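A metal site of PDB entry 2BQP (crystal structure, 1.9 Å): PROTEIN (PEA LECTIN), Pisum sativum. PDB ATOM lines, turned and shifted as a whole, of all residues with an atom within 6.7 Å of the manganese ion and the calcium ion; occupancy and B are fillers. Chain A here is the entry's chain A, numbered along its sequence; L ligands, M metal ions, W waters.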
ATOM      1  N   ASP A  81      19.848   5.845  29.783  1.00  0.00           N
ATOM      2  CA  ASP A  81      18.478   6.283  29.529  1.00  0.00           C
ATOM      3  C   ASP A  81      17.504   5.949  30.651  1.00  0.00           C
ATOM      4  O   ASP A  81      16.440   6.577  30.773  1.00  0.00           O
ATOM      5  CB  ASP A  81      17.962   5.649  28.254  1.00  0.00           C
ATOM      6  CG  ASP A  81      18.243   6.485  27.042  1.00  0.00           C
ATOM      7  OD1 ASP A  81      17.462   7.422  26.834  1.00  0.00           O
ATOM      8  OD2 ASP A  81      19.234   6.223  26.331  1.00  0.00           O
ATOM      9  N   GLY A  99      15.969   5.520  24.301  1.00  0.00           N
ATOM     10  CA  GLY A  99      14.834   6.103  24.994  1.00  0.00           C
ATOM     11  C   GLY A  99      13.659   5.191  25.180  1.00  0.00           C
ATOM     12  O   GLY A  99      12.827   5.466  26.026  1.00  0.00           O
ATOM     13  N   TYR A 100      13.582   4.116  24.401  1.00  0.00           N
ATOM     14  CA  TYR A 100      12.499   3.130  24.520  1.00  0.00           C
ATOM     15  C   TYR A 100      12.736   2.123  25.658  1.00  0.00           C
ATOM     16  O   TYR A 100      11.874   1.298  25.971  1.00  0.00           O
ATOM     17  CB  TYR A 100      12.292   2.412  23.188  1.00  0.00           C
ATOM     18  CG  TYR A 100      11.695   3.327  22.159  1.00  0.00           C
ATOM     19  CD1 TYR A 100      10.314   3.518  22.095  1.00  0.00           C
ATOM     20  CD2 TYR A 100      12.504   4.038  21.291  1.00  0.00           C
ATOM     21  CE1 TYR A 100       9.765   4.427  21.193  1.00  0.00           C
ATOM     22  CE2 TYR A 100      11.966   4.941  20.388  1.00  0.00           C
ATOM     23  CZ  TYR A 100      10.601   5.127  20.343  1.00  0.00           C
ATOM     24  OH  TYR A 100      10.066   6.020  19.429  1.00  0.00           O
ATOM     25  N   LEU A 101      13.925   2.195  26.253  1.00  0.00           N
ATOM     26  CA  LEU A 101      14.305   1.396  27.410  1.00  0.00           C
ATOM     27  C   LEU A 101      14.292  -0.110  27.222  1.00  0.00           C
ATOM     28  O   LEU A 101      14.242  -0.856  28.208  1.00  0.00           O
ATOM     29  CB  LEU A 101      13.440   1.819  28.616  1.00  0.00           C
ATOM     30  CG  LEU A 101      13.534   3.301  28.988  1.00  0.00           C
ATOM     31  CD1 LEU A 101      12.435   3.664  29.997  1.00  0.00           C
ATOM     32  CD2 LEU A 101      14.913   3.607  29.526  1.00  0.00           C
ATOM     33  N   GLU A 119       8.904   2.770  34.956  1.00  0.00           N
ATOM     34  CA  GLU A 119      10.190   3.329  34.570  1.00  0.00           C
ATOM     35  C   GLU A 119      10.841   4.326  35.498  1.00  0.00           C
ATOM     36  O   GLU A 119      10.165   5.046  36.242  1.00  0.00           O
ATOM     37  CB  GLU A 119      10.092   3.949  33.191  1.00  0.00           C
ATOM     38  CG  GLU A 119       9.143   5.178  33.150  1.00  0.00           C
ATOM     39  CD  GLU A 119       9.276   5.994  31.873  1.00  0.00           C
ATOM     40  OE1 GLU A 119       8.912   5.476  30.800  1.00  0.00           O
ATOM     41  OE2 GLU A 119       9.748   7.151  31.958  1.00  0.00           O
ATOM     42  N   ASP A 121      13.178   6.896  34.427  1.00  0.00           N
ATOM     43  CA  ASP A 121      13.664   7.549  33.242  1.00  0.00           C
ATOM     44  C   ASP A 121      14.605   8.687  33.573  1.00  0.00           C
ATOM     45  O   ASP A 121      14.193   9.699  34.151  1.00  0.00           O
ATOM     46  CB  ASP A 121      12.424   8.041  32.491  1.00  0.00           C
ATOM     47  CG  ASP A 121      12.718   8.543  31.118  1.00  0.00           C
ATOM     48  OD1 ASP A 121      13.890   8.840  30.813  1.00  0.00           O
ATOM     49  OD2 ASP A 121      11.727   8.708  30.354  1.00  0.00           O
ATOM     50  N   THR A 122      15.835   8.581  33.105  1.00  0.00           N
ATOM     51  CA  THR A 122      16.858   9.590  33.383  1.00  0.00           C
ATOM     52  C   THR A 122      17.194  10.572  32.261  1.00  0.00           C
ATOM     53  O   THR A 122      18.084  11.407  32.427  1.00  0.00           O
ATOM     54  CB  THR A 122      18.176   8.912  33.781  1.00  0.00           C
ATOM     55  OG1 THR A 122      18.585   8.015  32.746  1.00  0.00           O
ATOM     56  CG2 THR A 122      18.013   8.128  35.070  1.00  0.00           C
ATOM     57  N   PHE A 123      16.507  10.482  31.134  1.00  0.00           N
ATOM     58  CA  PHE A 123      16.821  11.340  29.998  1.00  0.00           C
ATOM     59  C   PHE A 123      15.557  11.803  29.321  1.00  0.00           C
ATOM     60  O   PHE A 123      14.697  10.998  28.940  1.00  0.00           O
ATOM     61  CB  PHE A 123      17.681  10.566  29.006  1.00  0.00           C
ATOM     62  CG  PHE A 123      18.015  11.325  27.741  1.00  0.00           C
ATOM     63  CD1 PHE A 123      19.134  12.134  27.685  1.00  0.00           C
ATOM     64  CD2 PHE A 123      17.226  11.190  26.616  1.00  0.00           C
ATOM     65  CE1 PHE A 123      19.473  12.788  26.523  1.00  0.00           C
ATOM     66  CE2 PHE A 123      17.555  11.841  25.446  1.00  0.00           C
ATOM     67  CZ  PHE A 123      18.687  12.644  25.399  1.00  0.00           C
ATOM     68  N   TYR A 124      15.495  13.114  29.091  1.00  0.00           N
ATOM     69  CA  TYR A 124      14.337  13.751  28.478  1.00  0.00           C
ATOM     70  C   TYR A 124      14.234  13.513  26.978  1.00  0.00           C
ATOM     71  O   TYR A 124      15.125  13.903  26.245  1.00  0.00           O
ATOM     72  CB  TYR A 124      14.396  15.252  28.782  1.00  0.00           C
ATOM     73  CG  TYR A 124      13.351  16.044  28.042  1.00  0.00           C
ATOM     74  CD1 TYR A 124      11.996  15.821  28.273  1.00  0.00           C
ATOM     75  CD2 TYR A 124      13.722  17.017  27.108  1.00  0.00           C
ATOM     76  CE1 TYR A 124      11.013  16.540  27.569  1.00  0.00           C
ATOM     77  CE2 TYR A 124      12.748  17.739  26.404  1.00  0.00           C
ATOM     78  CZ  TYR A 124      11.391  17.494  26.645  1.00  0.00           C
ATOM     79  OH  TYR A 124      10.412  18.203  25.952  1.00  0.00           O
ATOM     80  N   ASN A 125      13.196  12.806  26.541  1.00  0.00           N
ATOM     81  CA  ASN A 125      12.970  12.547  25.114  1.00  0.00           C
ATOM     82  C   ASN A 125      11.797  13.444  24.795  1.00  0.00           C
ATOM     83  O   ASN A 125      10.648  13.122  25.139  1.00  0.00           O
ATOM     84  CB  ASN A 125      12.595  11.095  24.799  1.00  0.00           C
ATOM     85  CG  ASN A 125      13.722  10.130  25.074  1.00  0.00           C
ATOM     86  OD1 ASN A 125      13.744   9.504  26.119  1.00  0.00           O
ATOM     87  ND2 ASN A 125      14.694  10.083  24.187  1.00  0.00           N
ATOM     88  N   TRP A 128       8.003  12.570  23.807  1.00  0.00           N
ATOM     89  CA  TRP A 128       6.995  11.981  24.700  1.00  0.00           C
ATOM     90  C   TRP A 128       7.157  12.207  26.214  1.00  0.00           C
ATOM     91  O   TRP A 128       6.196  11.993  26.959  1.00  0.00           O
ATOM     92  CB  TRP A 128       6.844  10.458  24.456  1.00  0.00           C
ATOM     93  CG  TRP A 128       8.121   9.682  24.750  1.00  0.00           C
ATOM     94  CD1 TRP A 128       8.651   9.400  25.985  1.00  0.00           C
ATOM     95  CD2 TRP A 128       9.064   9.202  23.790  1.00  0.00           C
ATOM     96  NE1 TRP A 128       9.856   8.789  25.849  1.00  0.00           N
ATOM     97  CE2 TRP A 128      10.141   8.653  24.519  1.00  0.00           C
ATOM     98  CE3 TRP A 128       9.100   9.181  22.400  1.00  0.00           C
ATOM     99  CZ2 TRP A 128      11.254   8.095  23.897  1.00  0.00           C
ATOM    100  CZ3 TRP A 128      10.188   8.635  21.780  1.00  0.00           C
ATOM    101  CH2 TRP A 128      11.266   8.087  22.529  1.00  0.00           C
ATOM    102  N   ASP A 129       8.361  12.559  26.668  1.00  0.00           N
ATOM    103  CA  ASP A 129       8.573  12.739  28.099  1.00  0.00           C
ATOM    104  C   ASP A 129       7.955  14.050  28.617  1.00  0.00           C
ATOM    105  O   ASP A 129       7.599  14.920  27.807  1.00  0.00           O
ATOM    106  CB  ASP A 129      10.066  12.703  28.417  1.00  0.00           C
ATOM    107  CG  ASP A 129      10.621  11.287  28.453  1.00  0.00           C
ATOM    108  OD1 ASP A 129       9.852  10.345  28.761  1.00  0.00           O
ATOM    109  OD2 ASP A 129      11.822  11.108  28.181  1.00  0.00           O
ATOM    110  N   PRO A 130       7.772  14.168  29.947  1.00  0.00           N
ATOM    111  CA  PRO A 130       7.204  15.369  30.574  1.00  0.00           C
ATOM    112  C   PRO A 130       7.937  16.657  30.147  1.00  0.00           C
ATOM    113  O   PRO A 130       9.175  16.724  30.205  1.00  0.00           O
ATOM    114  CB  PRO A 130       7.406  15.101  32.062  1.00  0.00           C
ATOM    115  CG  PRO A 130       7.208  13.669  32.161  1.00  0.00           C
ATOM    116  CD  PRO A 130       7.996  13.135  30.977  1.00  0.00           C
ATOM    117  N   HIS A 136      12.094  11.273  35.960  1.00  0.00           N
ATOM    118  CA  HIS A 136      10.864  10.914  36.605  1.00  0.00           C
ATOM    119  C   HIS A 136      10.651   9.412  36.738  1.00  0.00           C
ATOM    120  O   HIS A 136      11.344   8.614  36.095  1.00  0.00           O
ATOM    121  CB  HIS A 136       9.716  11.512  35.771  1.00  0.00           C
ATOM    122  CG  HIS A 136       9.864  11.265  34.298  1.00  0.00           C
ATOM    123  ND1 HIS A 136      10.825  11.870  33.520  1.00  0.00           N
ATOM    124  CD2 HIS A 136       9.209  10.404  33.476  1.00  0.00           C
ATOM    125  CE1 HIS A 136      10.766  11.404  32.295  1.00  0.00           C
ATOM    126  NE2 HIS A 136       9.779  10.514  32.231  1.00  0.00           N
ATOM    127  N   GLY A 138       7.608   6.661  36.224  1.00  0.00           N
ATOM    128  CA  GLY A 138       6.399   6.646  35.428  1.00  0.00           C
ATOM    129  C   GLY A 138       5.837   5.268  35.289  1.00  0.00           C
ATOM    130  O   GLY A 138       6.540   4.273  35.476  1.00  0.00           O
ATOM    131  N   ASP A 140       4.070   2.870  32.678  1.00  0.00           N
ATOM    132  CA  ASP A 140       3.834   2.671  31.251  1.00  0.00           C
ATOM    133  C   ASP A 140       2.942   1.465  30.967  1.00  0.00           C
ATOM    134  O   ASP A 140       3.067   0.408  31.605  1.00  0.00           O
ATOM    135  CB  ASP A 140       5.177   2.498  30.543  1.00  0.00           C
ATOM    136  CG  ASP A 140       6.154   3.617  30.841  1.00  0.00           C
ATOM    137  OD1 ASP A 140       5.735   4.679  31.328  1.00  0.00           O
ATOM    138  OD2 ASP A 140       7.359   3.461  30.579  1.00  0.00           O
ATOM    139  N   ILE A 144       5.679   3.977  25.487  1.00  0.00           N
ATOM    140  CA  ILE A 144       6.774   4.587  26.244  1.00  0.00           C
ATOM    141  C   ILE A 144       6.332   5.938  26.843  1.00  0.00           C
ATOM    142  O   ILE A 144       7.073   6.543  27.645  1.00  0.00           O
ATOM    143  CB  ILE A 144       8.064   4.766  25.378  1.00  0.00           C
ATOM    144  CG1 ILE A 144       9.281   5.070  26.284  1.00  0.00           C
ATOM    145  CG2 ILE A 144       7.895   5.892  24.360  1.00  0.00           C
ATOM    146  CD1 ILE A 144       9.622   3.983  27.344  1.00  0.00           C
ATOM    147  N   LYS A 145       5.158   6.411  26.438  1.00  0.00           N
ATOM    148  CA  LYS A 145       4.635   7.670  26.979  1.00  0.00           C
ATOM    149  C   LYS A 145       3.806   7.248  28.190  1.00  0.00           C
ATOM    150  O   LYS A 145       2.721   6.705  28.033  1.00  0.00           O
ATOM    151  CB  LYS A 145       3.741   8.366  25.956  1.00  0.00           C
ATOM    152  CG  LYS A 145       3.477   9.819  26.273  1.00  0.00           C
ATOM    153  CD  LYS A 145       2.370  10.379  25.397  1.00  0.00           C
ATOM    154  CE  LYS A 145       2.279  11.891  25.534  1.00  0.00           C
ATOM    155  NZ  LYS A 145       3.459  12.561  24.914  1.00  0.00           N
ATOM    156  N   SER A 146       4.359   7.471  29.375  1.00  0.00           N
ATOM    157  CA  SER A 146       3.725   7.085  30.636  1.00  0.00           C
ATOM    158  C   SER A 146       2.295   7.566  30.829  1.00  0.00           C
ATOM    159  O   SER A 146       1.923   8.611  30.327  1.00  0.00           O
ATOM    160  CB  SER A 146       4.572   7.590  31.803  1.00  0.00           C
ATOM    161  OG  SER A 146       5.960   7.401  31.554  1.00  0.00           O
ATOM    162  N   THR A 149       3.364  10.181  35.722  1.00  0.00           N
ATOM    163  CA  THR A 149       4.787  10.291  36.052  1.00  0.00           C
ATOM    164  C   THR A 149       4.945  11.129  37.314  1.00  0.00           C
ATOM    165  O   THR A 149       3.994  11.775  37.747  1.00  0.00           O
ATOM    166  CB  THR A 149       5.600  10.972  34.934  1.00  0.00           C
ATOM    167  OG1 THR A 149       5.250  12.363  34.849  1.00  0.00           O
ATOM    168  CG2 THR A 149       5.315  10.322  33.587  1.00  0.00           C
HETATM  169  C1  LIG L   1      19.929   8.932  21.274  1.00  0.00           C
HETATM  170  C2  LIG L   1      18.836   7.889  21.125  1.00  0.00           C
HETATM  171  C3  LIG L   1      17.733   8.198  22.116  1.00  0.00           C
HETATM  172  C4  LIG L   1      18.293   8.254  23.528  1.00  0.00           C
HETATM  173  C5  LIG L   1      19.443   9.253  23.582  1.00  0.00           C
HETATM  174  C6  LIG L   1      20.134   9.345  24.939  1.00  0.00           C
HETATM  175  O1  LIG L   1      20.947   8.658  20.390  1.00  0.00           O
HETATM  176  O2  LIG L   1      18.341   7.918  19.795  1.00  0.00           O
HETATM  177  O3  LIG L   1      16.732   7.197  22.067  1.00  0.00           O
HETATM  178  O4  LIG L   1      17.263   8.652  24.408  1.00  0.00           O
HETATM  179  O5  LIG L   1      20.447   8.900  22.612  1.00  0.00           O
HETATM  180  O6  LIG L   1      20.980   8.229  25.177  1.00  0.00           O
HETATM  181 MN    MN M   1       9.715   8.820  30.395  1.00  0.00          MN
HETATM  182 CA    CA M   2      13.466   9.305  28.495  1.00  0.00          CA
HETATM  183  O   HOH W   1       8.010   8.994  30.716  1.00  0.00           O
HETATM  184  O   HOH W   2      15.254   8.007  28.607  1.00  0.00           O
HETATM  185  O   HOH W   3       9.324   7.340  28.966  1.00  0.00           O
HETATM  186  O   HOH W   4      12.242   7.836  27.650  1.00  0.00           O
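The side-chain amide nitrogen (ND2) of Asn 125 lies within hydrogen-bond range of an oxygen (O4) of the ligand. The backbone NH (N) of Gly 99 is in hydrogen-bond range of an oxygen (O3) of the ligand (2.9 Å). The side-chain carboxylate of Asp 81 lies within hydrogen-bond range of an oxygen (O4) of the ligand (2.7 Å).
OD1 of Asp 129 sits close to NE1 of Trp 128, 3.3 Å away. The side-chain carboxylate (OD2) of Asp 140 lies close to the side-chain carboxylate (OE1) of Glu 119. O of Gly 138 lies within hydrogen-bond range of N of Glu 119 (2.8 Å).
Four residues have an atom within 4 Å of the manganese ion: Glu 119, Asp 121, Asp 129 and His 136.
Of the 20 residues printed, 4 come within 4 Å of the calcium ion. The nearest printed residue that does not touch the calcium ion is Tyr 124 (4.4 Å).
The manganese ion is bound by water W1 (1.7 Å), OD2 of Asp 121 (2.0 Å), water W3 (2.1 Å), OD1 of Asp 129 (2.2 Å), OE2 of Glu 119 (2.3 Å) and NE2 of His 136 (2.5 Å). The manganese ion has six donor atoms within binding distance.
The calcium ion is bound by water W4 (2.1 Å), O of Phe 123 (2.1 Å), water W2 (2.2 Å), OD1 of Asn 125 (2.4 Å), OD1 of Asp 121 (2.4 Å), OD2 of Asp 129 (2.5 Å) and OD2 of Asp 121 (2.6 Å). The calcium ion has seven donor atoms within binding distance.
Water W3 lies within hydrogen-bond range of the side-chain carboxylate of Glu 119 (2.6 Å), the backbone carbonyl oxygen of Ile 144 (2.7 Å) and the indole nitrogen of Trp 128 (3.5 Å). Water W4 lies within hydrogen-bond range of O of Gly 99 (2.9 Å) and NE1 of Trp 128 (3.1 Å).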
